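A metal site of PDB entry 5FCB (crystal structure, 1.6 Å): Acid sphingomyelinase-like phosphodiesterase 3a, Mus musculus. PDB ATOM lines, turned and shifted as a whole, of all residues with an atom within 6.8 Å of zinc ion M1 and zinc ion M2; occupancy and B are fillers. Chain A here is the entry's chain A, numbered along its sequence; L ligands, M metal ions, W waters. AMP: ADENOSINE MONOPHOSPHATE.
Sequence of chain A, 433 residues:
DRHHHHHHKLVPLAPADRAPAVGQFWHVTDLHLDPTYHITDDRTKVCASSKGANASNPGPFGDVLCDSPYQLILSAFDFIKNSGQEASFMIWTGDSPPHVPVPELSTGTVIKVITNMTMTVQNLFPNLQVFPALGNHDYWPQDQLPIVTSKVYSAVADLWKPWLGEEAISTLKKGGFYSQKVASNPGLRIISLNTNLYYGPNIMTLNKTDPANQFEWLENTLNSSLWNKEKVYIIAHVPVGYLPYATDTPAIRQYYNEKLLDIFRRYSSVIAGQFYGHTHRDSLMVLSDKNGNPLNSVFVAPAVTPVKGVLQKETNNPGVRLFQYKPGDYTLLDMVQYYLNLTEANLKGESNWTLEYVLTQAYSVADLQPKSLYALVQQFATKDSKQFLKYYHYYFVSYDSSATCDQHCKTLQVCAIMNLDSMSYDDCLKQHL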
ATOM      1  N   THR A  29      13.959 -19.936  -0.879  1.00  0.00           N
ATOM      2  CA  THR A  29      13.439 -20.548  -2.087  1.00  0.00           C
ATOM      3  C   THR A  29      14.578 -21.133  -2.926  1.00  0.00           C
ATOM      4  O   THR A  29      15.727 -20.698  -2.833  1.00  0.00           O
ATOM      5  CB  THR A  29      12.629 -19.519  -2.897  1.00  0.00           C
ATOM      6  OG1 THR A  29      11.891 -20.182  -3.924  1.00  0.00           O
ATOM      7  CG2 THR A  29      13.514 -18.438  -3.486  1.00  0.00           C
ATOM      8  N   ASP A  30      14.220 -22.121  -3.735  1.00  0.00           N
ATOM      9  CA  ASP A  30      15.086 -22.636  -4.799  1.00  0.00           C
ATOM     10  C   ASP A  30      16.421 -23.130  -4.245  1.00  0.00           C
ATOM     11  O   ASP A  30      17.496 -22.686  -4.636  1.00  0.00           O
ATOM     12  CB  ASP A  30      15.269 -21.570  -5.892  1.00  0.00           C
ATOM     13  CG  ASP A  30      13.973 -21.326  -6.666  1.00  0.00           C
ATOM     14  OD1 ASP A  30      13.224 -20.408  -6.286  1.00  0.00           O
ATOM     15  OD2 ASP A  30      13.721 -22.100  -7.615  1.00  0.00           O
ATOM     16  N   LEU A  31      16.306 -24.074  -3.301  1.00  0.00           N
ATOM     17  CA  LEU A  31      17.475 -24.641  -2.657  1.00  0.00           C
ATOM     18  C   LEU A  31      18.287 -25.498  -3.613  1.00  0.00           C
ATOM     19  O   LEU A  31      19.520 -25.459  -3.581  1.00  0.00           O
ATOM     20  CB  LEU A  31      17.036 -25.458  -1.442  1.00  0.00           C
ATOM     21  CG  LEU A  31      16.267 -24.689  -0.370  1.00  0.00           C
ATOM     22  CD1 LEU A  31      15.754 -25.632   0.693  1.00  0.00           C
ATOM     23  CD2 LEU A  31      17.118 -23.618   0.254  1.00  0.00           C
ATOM     24  N   HIS A  32      17.617 -26.283  -4.465  1.00  0.00           N
ATOM     25  CA  HIS A  32      18.243 -27.107  -5.508  1.00  0.00           C
ATOM     26  C   HIS A  32      19.497 -27.821  -4.980  1.00  0.00           C
ATOM     27  O   HIS A  32      20.609 -27.600  -5.463  1.00  0.00           O
ATOM     28  CB  HIS A  32      18.587 -26.276  -6.748  1.00  0.00           C
ATOM     29  CG  HIS A  32      17.389 -25.790  -7.521  1.00  0.00           C
ATOM     30  ND1 HIS A  32      16.562 -26.634  -8.235  1.00  0.00           N
ATOM     31  CD2 HIS A  32      16.925 -24.536  -7.721  1.00  0.00           C
ATOM     32  CE1 HIS A  32      15.628 -25.918  -8.830  1.00  0.00           C
ATOM     33  NE2 HIS A  32      15.826 -24.643  -8.536  1.00  0.00           N
ATOM     34  N   GLY A  94       9.859 -23.632  -2.798  1.00  0.00           N
ATOM     35  CA  GLY A  94       9.983 -24.803  -3.649  1.00  0.00           C
ATOM     36  C   GLY A  94      11.317 -24.924  -4.377  1.00  0.00           C
ATOM     37  O   GLY A  94      12.245 -24.139  -4.200  1.00  0.00           O
ATOM     38  N   ASP A  95      11.362 -25.997  -5.198  1.00  0.00           N
ATOM     39  CA  ASP A  95      12.464 -26.350  -6.107  1.00  0.00           C
ATOM     40  C   ASP A  95      13.665 -26.918  -5.373  1.00  0.00           C
ATOM     41  O   ASP A  95      14.719 -26.265  -5.265  1.00  0.00           O
ATOM     42  CB  ASP A  95      12.864 -25.147  -6.981  1.00  0.00           C
ATOM     43  CG  ASP A  95      12.373 -25.290  -8.424  1.00  0.00           C
ATOM     44  OD1 ASP A  95      11.522 -26.162  -8.678  1.00  0.00           O
ATOM     45  OD2 ASP A  95      12.825 -24.502  -9.295  1.00  0.00           O
ATOM     46  N   SER A  96      13.541 -28.156  -4.919  1.00  0.00           N
ATOM     47  CA  SER A  96      14.578 -28.765  -4.097  1.00  0.00           C
ATOM     48  C   SER A  96      15.518 -29.725  -4.839  1.00  0.00           C
ATOM     49  O   SER A  96      16.708 -29.717  -4.532  1.00  0.00           O
ATOM     50  CB  SER A  96      13.939 -29.476  -2.910  1.00  0.00           C
ATOM     51  OG  SER A  96      13.381 -28.529  -2.016  1.00  0.00           O
ATOM     52  N   PRO A  97      15.055 -30.534  -5.796  1.00  0.00           N
ATOM     53  CA  PRO A  97      15.994 -31.384  -6.577  1.00  0.00           C
ATOM     54  C   PRO A  97      16.854 -30.551  -7.520  1.00  0.00           C
ATOM     55  O   PRO A  97      16.500 -29.407  -7.858  1.00  0.00           O
ATOM     56  CB  PRO A  97      15.053 -32.317  -7.363  1.00  0.00           C
ATOM     57  CG  PRO A  97      13.753 -32.287  -6.614  1.00  0.00           C
ATOM     58  CD  PRO A  97      13.658 -30.875  -6.097  1.00  0.00           C
ATOM     59  N   HIS A  99      19.134 -29.512 -11.079  1.00  0.00           N
ATOM     60  CA  HIS A  99      18.952 -29.458 -12.530  1.00  0.00           C
ATOM     61  C   HIS A  99      19.815 -30.525 -13.182  1.00  0.00           C
ATOM     62  O   HIS A  99      20.988 -30.297 -13.533  1.00  0.00           O
ATOM     63  CB  HIS A  99      19.326 -28.074 -13.075  1.00  0.00           C
ATOM     64  CG  HIS A  99      18.521 -26.939 -12.503  1.00  0.00           C
ATOM     65  ND1 HIS A  99      18.771 -26.386 -11.271  1.00  0.00           N
ATOM     66  CD2 HIS A  99      17.488 -26.243 -13.030  1.00  0.00           C
ATOM     67  CE1 HIS A  99      17.927 -25.396 -11.051  1.00  0.00           C
ATOM     68  NE2 HIS A  99      17.133 -25.281 -12.107  1.00  0.00           N
ATOM     69  N   GLY A 135       7.683 -26.464  -6.181  1.00  0.00           N
ATOM     70  CA  GLY A 135       8.261 -25.910  -7.390  1.00  0.00           C
ATOM     71  C   GLY A 135       8.169 -26.899  -8.549  1.00  0.00           C
ATOM     72  O   GLY A 135       7.757 -28.049  -8.412  1.00  0.00           O
ATOM     73  N   ASN A 136       8.559 -26.419  -9.739  1.00  0.00           N
ATOM     74  CA  ASN A 136       8.410 -27.252 -10.932  1.00  0.00           C
ATOM     75  C   ASN A 136       9.387 -28.422 -10.948  1.00  0.00           C
ATOM     76  O   ASN A 136       9.110 -29.434 -11.600  1.00  0.00           O
ATOM     77  CB  ASN A 136       8.547 -26.401 -12.190  1.00  0.00           C
ATOM     78  CG  ASN A 136       9.827 -25.612 -12.229  1.00  0.00           C
ATOM     79  OD1 ASN A 136      10.062 -24.747 -11.385  1.00  0.00           O
ATOM     80  ND2 ASN A 136      10.660 -25.886 -13.230  1.00  0.00           N
ATOM     81  N   HIS A 137      10.514 -28.331 -10.251  1.00  0.00           N
ATOM     82  CA  HIS A 137      11.415 -29.463 -10.116  1.00  0.00           C
ATOM     83  C   HIS A 137      11.023 -30.414  -8.995  1.00  0.00           C
ATOM     84  O   HIS A 137      11.666 -31.465  -8.858  1.00  0.00           O
ATOM     85  CB  HIS A 137      12.839 -28.971  -9.868  1.00  0.00           C
ATOM     86  CG  HIS A 137      13.446 -28.328 -11.063  1.00  0.00           C
ATOM     87  ND1 HIS A 137      14.177 -29.029 -12.010  1.00  0.00           N
ATOM     88  CD2 HIS A 137      13.389 -27.048 -11.519  1.00  0.00           C
ATOM     89  CE1 HIS A 137      14.569 -28.204 -12.961  1.00  0.00           C
ATOM     90  NE2 HIS A 137      14.104 -27.000 -12.691  1.00  0.00           N
ATOM     91  N   ASP A 143       8.380 -30.523 -14.058  1.00  0.00           N
ATOM     92  CA  ASP A 143       7.387 -29.658 -14.673  1.00  0.00           C
ATOM     93  C   ASP A 143       6.050 -30.351 -14.895  1.00  0.00           C
ATOM     94  O   ASP A 143       5.071 -29.662 -15.192  1.00  0.00           O
ATOM     95  CB  ASP A 143       7.869 -29.082 -16.022  1.00  0.00           C
ATOM     96  CG  ASP A 143       9.249 -28.458 -15.939  1.00  0.00           C
ATOM     97  OD1 ASP A 143       9.610 -27.952 -14.858  1.00  0.00           O
ATOM     98  OD2 ASP A 143       9.973 -28.471 -16.958  1.00  0.00           O
ATOM     99  N   ASN A 196       2.817 -24.187 -10.752  1.00  0.00           N
ATOM    100  CA  ASN A 196       3.375 -25.089 -11.741  1.00  0.00           C
ATOM    101  C   ASN A 196       2.285 -25.674 -12.627  1.00  0.00           C
ATOM    102  O   ASN A 196       2.591 -26.099 -13.744  1.00  0.00           O
ATOM    103  CB  ASN A 196       4.163 -26.194 -11.042  1.00  0.00           C
ATOM    104  CG  ASN A 196       5.077 -25.636  -9.989  1.00  0.00           C
ATOM    105  OD1 ASN A 196       6.064 -24.980 -10.307  1.00  0.00           O
ATOM    106  ND2 ASN A 196       4.718 -25.840  -8.728  1.00  0.00           N
ATOM    107  N   TYR A 199       2.491 -23.518 -15.685  1.00  0.00           N
ATOM    108  CA  TYR A 199       3.817 -23.302 -16.248  1.00  0.00           C
ATOM    109  C   TYR A 199       3.899 -23.962 -17.625  1.00  0.00           C
ATOM    110  O   TYR A 199       3.459 -25.104 -17.807  1.00  0.00           O
ATOM    111  CB  TYR A 199       4.840 -23.858 -15.258  1.00  0.00           C
ATOM    112  CG  TYR A 199       6.289 -23.707 -15.621  1.00  0.00           C
ATOM    113  CD1 TYR A 199       6.823 -22.475 -15.982  1.00  0.00           C
ATOM    114  CD2 TYR A 199       7.142 -24.797 -15.516  1.00  0.00           C
ATOM    115  CE1 TYR A 199       8.167 -22.356 -16.270  1.00  0.00           C
ATOM    116  CE2 TYR A 199       8.475 -24.684 -15.809  1.00  0.00           C
ATOM    117  CZ  TYR A 199       8.990 -23.463 -16.192  1.00  0.00           C
ATOM    118  OH  TYR A 199      10.332 -23.365 -16.472  1.00  0.00           O
ATOM    119  N   HIS A 237       5.582 -20.855  -6.339  1.00  0.00           N
ATOM    120  CA  HIS A 237       6.889 -20.977  -6.979  1.00  0.00           C
ATOM    121  C   HIS A 237       7.003 -20.063  -8.205  1.00  0.00           C
ATOM    122  O   HIS A 237       7.737 -19.065  -8.176  1.00  0.00           O
ATOM    123  CB  HIS A 237       7.151 -22.436  -7.386  1.00  0.00           C
ATOM    124  CG  HIS A 237       8.519 -22.625  -7.934  1.00  0.00           C
ATOM    125  ND1 HIS A 237       9.650 -22.432  -7.174  1.00  0.00           N
ATOM    126  CD2 HIS A 237       8.954 -22.913  -9.184  1.00  0.00           C
ATOM    127  CE1 HIS A 237      10.724 -22.610  -7.929  1.00  0.00           C
ATOM    128  NE2 HIS A 237      10.332 -22.907  -9.152  1.00  0.00           N
ATOM    129  N   VAL A 238       6.326 -20.412  -9.289  1.00  0.00           N
ATOM    130  CA  VAL A 238       6.400 -19.597 -10.510  1.00  0.00           C
ATOM    131  C   VAL A 238       5.576 -18.333 -10.315  1.00  0.00           C
ATOM    132  O   VAL A 238       4.414 -18.416  -9.861  1.00  0.00           O
ATOM    133  CB  VAL A 238       5.916 -20.372 -11.730  1.00  0.00           C
ATOM    134  CG1 VAL A 238       6.165 -19.551 -13.009  1.00  0.00           C
ATOM    135  CG2 VAL A 238       6.585 -21.737 -11.829  1.00  0.00           C
ATOM    136  N   GLY A 277       9.207 -17.431  -6.139  1.00  0.00           N
ATOM    137  CA  GLY A 277      10.597 -17.775  -6.438  1.00  0.00           C
ATOM    138  C   GLY A 277      10.791 -18.068  -7.910  1.00  0.00           C
ATOM    139  O   GLY A 277      10.385 -17.258  -8.753  1.00  0.00           O
ATOM    140  N   HIS A 278      11.413 -19.214  -8.227  1.00  0.00           N
ATOM    141  CA  HIS A 278      11.572 -19.745  -9.589  1.00  0.00           C
ATOM    142  C   HIS A 278      12.576 -18.997 -10.467  1.00  0.00           C
ATOM    143  O   HIS A 278      13.357 -19.641 -11.182  1.00  0.00           O
ATOM    144  CB  HIS A 278      10.205 -19.817 -10.302  1.00  0.00           C
ATOM    145  CG  HIS A 278      10.292 -20.318 -11.704  1.00  0.00           C
ATOM    146  ND1 HIS A 278      10.616 -21.625 -12.019  1.00  0.00           N
ATOM    147  CD2 HIS A 278      10.115 -19.681 -12.878  1.00  0.00           C
ATOM    148  CE1 HIS A 278      10.627 -21.766 -13.339  1.00  0.00           C
ATOM    149  NE2 HIS A 278      10.332 -20.600 -13.877  1.00  0.00           N
ATOM    150  N   THR A 279      12.574 -17.651 -10.459  1.00  0.00           N
ATOM    151  CA  THR A 279      13.476 -16.934 -11.354  1.00  0.00           C
ATOM    152  C   THR A 279      14.896 -16.876 -10.848  1.00  0.00           C
ATOM    153  O   THR A 279      15.806 -16.542 -11.621  1.00  0.00           O
ATOM    154  CB  THR A 279      13.034 -15.491 -11.572  1.00  0.00           C
ATOM    155  OG1 THR A 279      13.237 -14.768 -10.373  1.00  0.00           O
ATOM    156  CG2 THR A 279      11.571 -15.437 -11.989  1.00  0.00           C
ATOM    157  N   HIS A 280      15.113 -17.160  -9.566  1.00  0.00           N
ATOM    158  CA  HIS A 280      16.421 -17.093  -8.930  1.00  0.00           C
ATOM    159  C   HIS A 280      16.992 -15.687  -8.904  1.00  0.00           C
ATOM    160  O   HIS A 280      18.207 -15.500  -8.760  1.00  0.00           O
ATOM    161  CB  HIS A 280      17.418 -18.043  -9.619  1.00  0.00           C
ATOM    162  CG  HIS A 280      17.071 -19.495  -9.534  1.00  0.00           C
ATOM    163  ND1 HIS A 280      18.001 -20.485  -9.743  1.00  0.00           N
ATOM    164  CD2 HIS A 280      15.896 -20.126  -9.287  1.00  0.00           C
ATOM    165  CE1 HIS A 280      17.413 -21.672  -9.637  1.00  0.00           C
ATOM    166  NE2 HIS A 280      16.137 -21.485  -9.349  1.00  0.00           N
ATOM    167  N   ALA A 303      17.415 -17.163  -5.303  1.00  0.00           N
ATOM    168  CA  ALA A 303      17.645 -18.545  -4.900  1.00  0.00           C
ATOM    169  C   ALA A 303      18.835 -18.668  -3.948  1.00  0.00           C
ATOM    170  O   ALA A 303      19.725 -17.812  -3.883  1.00  0.00           O
ATOM    171  CB  ALA A 303      17.888 -19.405  -6.121  1.00  0.00           C
ATOM    172  N   THR A 305      20.656 -21.580  -4.494  1.00  0.00           N
ATOM    173  CA  THR A 305      21.589 -22.049  -5.510  1.00  0.00           C
ATOM    174  C   THR A 305      22.100 -20.889  -6.366  1.00  0.00           C
ATOM    175  O   THR A 305      21.339 -19.949  -6.667  1.00  0.00           O
ATOM    176  CB  THR A 305      20.956 -23.113  -6.412  1.00  0.00           C
ATOM    177  OG1 THR A 305      21.934 -23.603  -7.347  1.00  0.00           O
ATOM    178  CG2 THR A 305      19.774 -22.563  -7.214  1.00  0.00           C
HETATM  179  P   AMP L   1      14.057 -23.805 -13.041  1.00  0.00           P
HETATM  180  O1P AMP L   1      14.538 -24.862 -14.013  1.00  0.00           O
HETATM  181  O2P AMP L   1      15.084 -23.505 -11.962  1.00  0.00           O
HETATM  182  O3P AMP L   1      12.644 -23.999 -12.531  1.00  0.00           O
HETATM  183  O5' AMP L   1      13.996 -22.523 -13.981  1.00  0.00           O
HETATM  184  C5' AMP L   1      15.062 -22.255 -14.869  1.00  0.00           C
HETATM  185  C4' AMP L   1      14.675 -22.342 -16.327  1.00  0.00           C
HETATM  186  O4' AMP L   1      14.546 -20.993 -16.847  1.00  0.00           O
HETATM  187  C3' AMP L   1      15.701 -23.021 -17.213  1.00  0.00           C
HETATM  188  O3' AMP L   1      15.068 -23.506 -18.400  1.00  0.00           O
HETATM  189  C2' AMP L   1      16.631 -21.869 -17.551  1.00  0.00           C
HETATM  190  O2' AMP L   1      17.424 -22.062 -18.713  1.00  0.00           O
HETATM  191  C1' AMP L   1      15.658 -20.699 -17.695  1.00  0.00           C
HETATM  192  N9  AMP L   1      16.198 -19.403 -17.268  1.00  0.00           N
HETATM  193  C8  AMP L   1      15.992 -18.866 -16.048  1.00  0.00           C
HETATM  194  N7  AMP L   1      16.592 -17.663 -15.904  1.00  0.00           N
HETATM  195  C5  AMP L   1      17.209 -17.400 -17.070  1.00  0.00           C
HETATM  196  C6  AMP L   1      18.010 -16.277 -17.574  1.00  0.00           C
HETATM  197  N6  AMP L   1      18.255 -15.229 -16.754  1.00  0.00           N
HETATM  198  N1  AMP L   1      18.475 -16.361 -18.840  1.00  0.00           N
HETATM  199  C2  AMP L   1      18.217 -17.428 -19.626  1.00  0.00           C
HETATM  200  N3  AMP L   1      17.479 -18.484 -19.216  1.00  0.00           N
HETATM  201  C4  AMP L   1      16.946 -18.538 -17.976  1.00  0.00           C
HETATM  202 ZN    ZN M   1      14.625 -23.049  -9.193  1.00  0.00          ZN
HETATM  203 ZN    ZN M   2      11.520 -23.287 -10.828  1.00  0.00          ZN
HETATM  204  O   HOH W   1      13.416 -22.270 -10.642  1.00  0.00           O
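Zinc ion M1 is bound by water W1 (2.0 Å). OD2 of Asp 30 binds zinc ion M1, 2.1 Å away. A ring nitrogen (NE2) of His 32 is bound to zinc ion M1 (2.1 Å). NE2 of His 280 binds zinc ion M1 (2.2 Å). Zinc ion M1 is bound by OD2 of Asp 95 (2.3 Å). Slightly farther from zinc ion M1 lies O2P of the ligand (2.8 Å).
The side-chain carboxylate of Asp 30 is in hydrogen-bond range of the backbone NH of His 278 (2.9 Å). O of Asp 30 sits at hydrogen-bond distance from N of Thr 305 (3.4 Å). OG1 of Thr 29 sits at hydrogen-bond distance from OD1 of Asp 30, at 2.7 Å. The backbone carbonyl oxygen of His 237 is in hydrogen-bond range of the backbone NH of Gly 277 (3.0 Å). A ring nitrogen (ND1) of His 32 lies within hydrogen-bond range of the backbone carbonyl oxygen (O) of Pro 97 (2.8 Å). OD1 of Asn 196 lies within hydrogen-bond range of N of Asn 136 (2.9 Å). OD1 of Asp 95 is in hydrogen-bond range of N of His 137 (2.9 Å). O of Asp 95 sits at hydrogen-bond distance from N of Leu 31 (3.3 Å).
Of the 23 residues printed, 4 come within 4 Å of zinc ion M1. Along chain A the residues within 4 Å of zinc ion M1 span positions 30 to 280.
A ring nitrogen (NE2) of His 280 lies close to an oxygen (O2P) of the ligand, at 3.5 Å. NE2 of His 137 is in hydrogen-bond range of O1P of the ligand (2.6 Å). NE2 of His 99 sits at hydrogen-bond distance from O2P of the ligand, at 2.7 Å.
Zinc ion M2 is bound by NE2 of His 237 (2.1 Å), OD1 of Asn 136 (2.1 Å), water W1 (2.2 Å), O3P of the ligand (2.2 Å), ND1 of His 278 (2.2 Å) and OD2 of Asp 95 (2.4 Å). Zinc ion M2 has six donor atoms within binding distance.
Water W1 lies within hydrogen-bond range of an oxygen (O2P) of the ligand (2.5 Å) and the backbone carbonyl oxygen (O) of His 278 (2.7 Å).
The nearest printed residue that does not touch zinc ion M2 is Asp 30 (4.1 Å).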
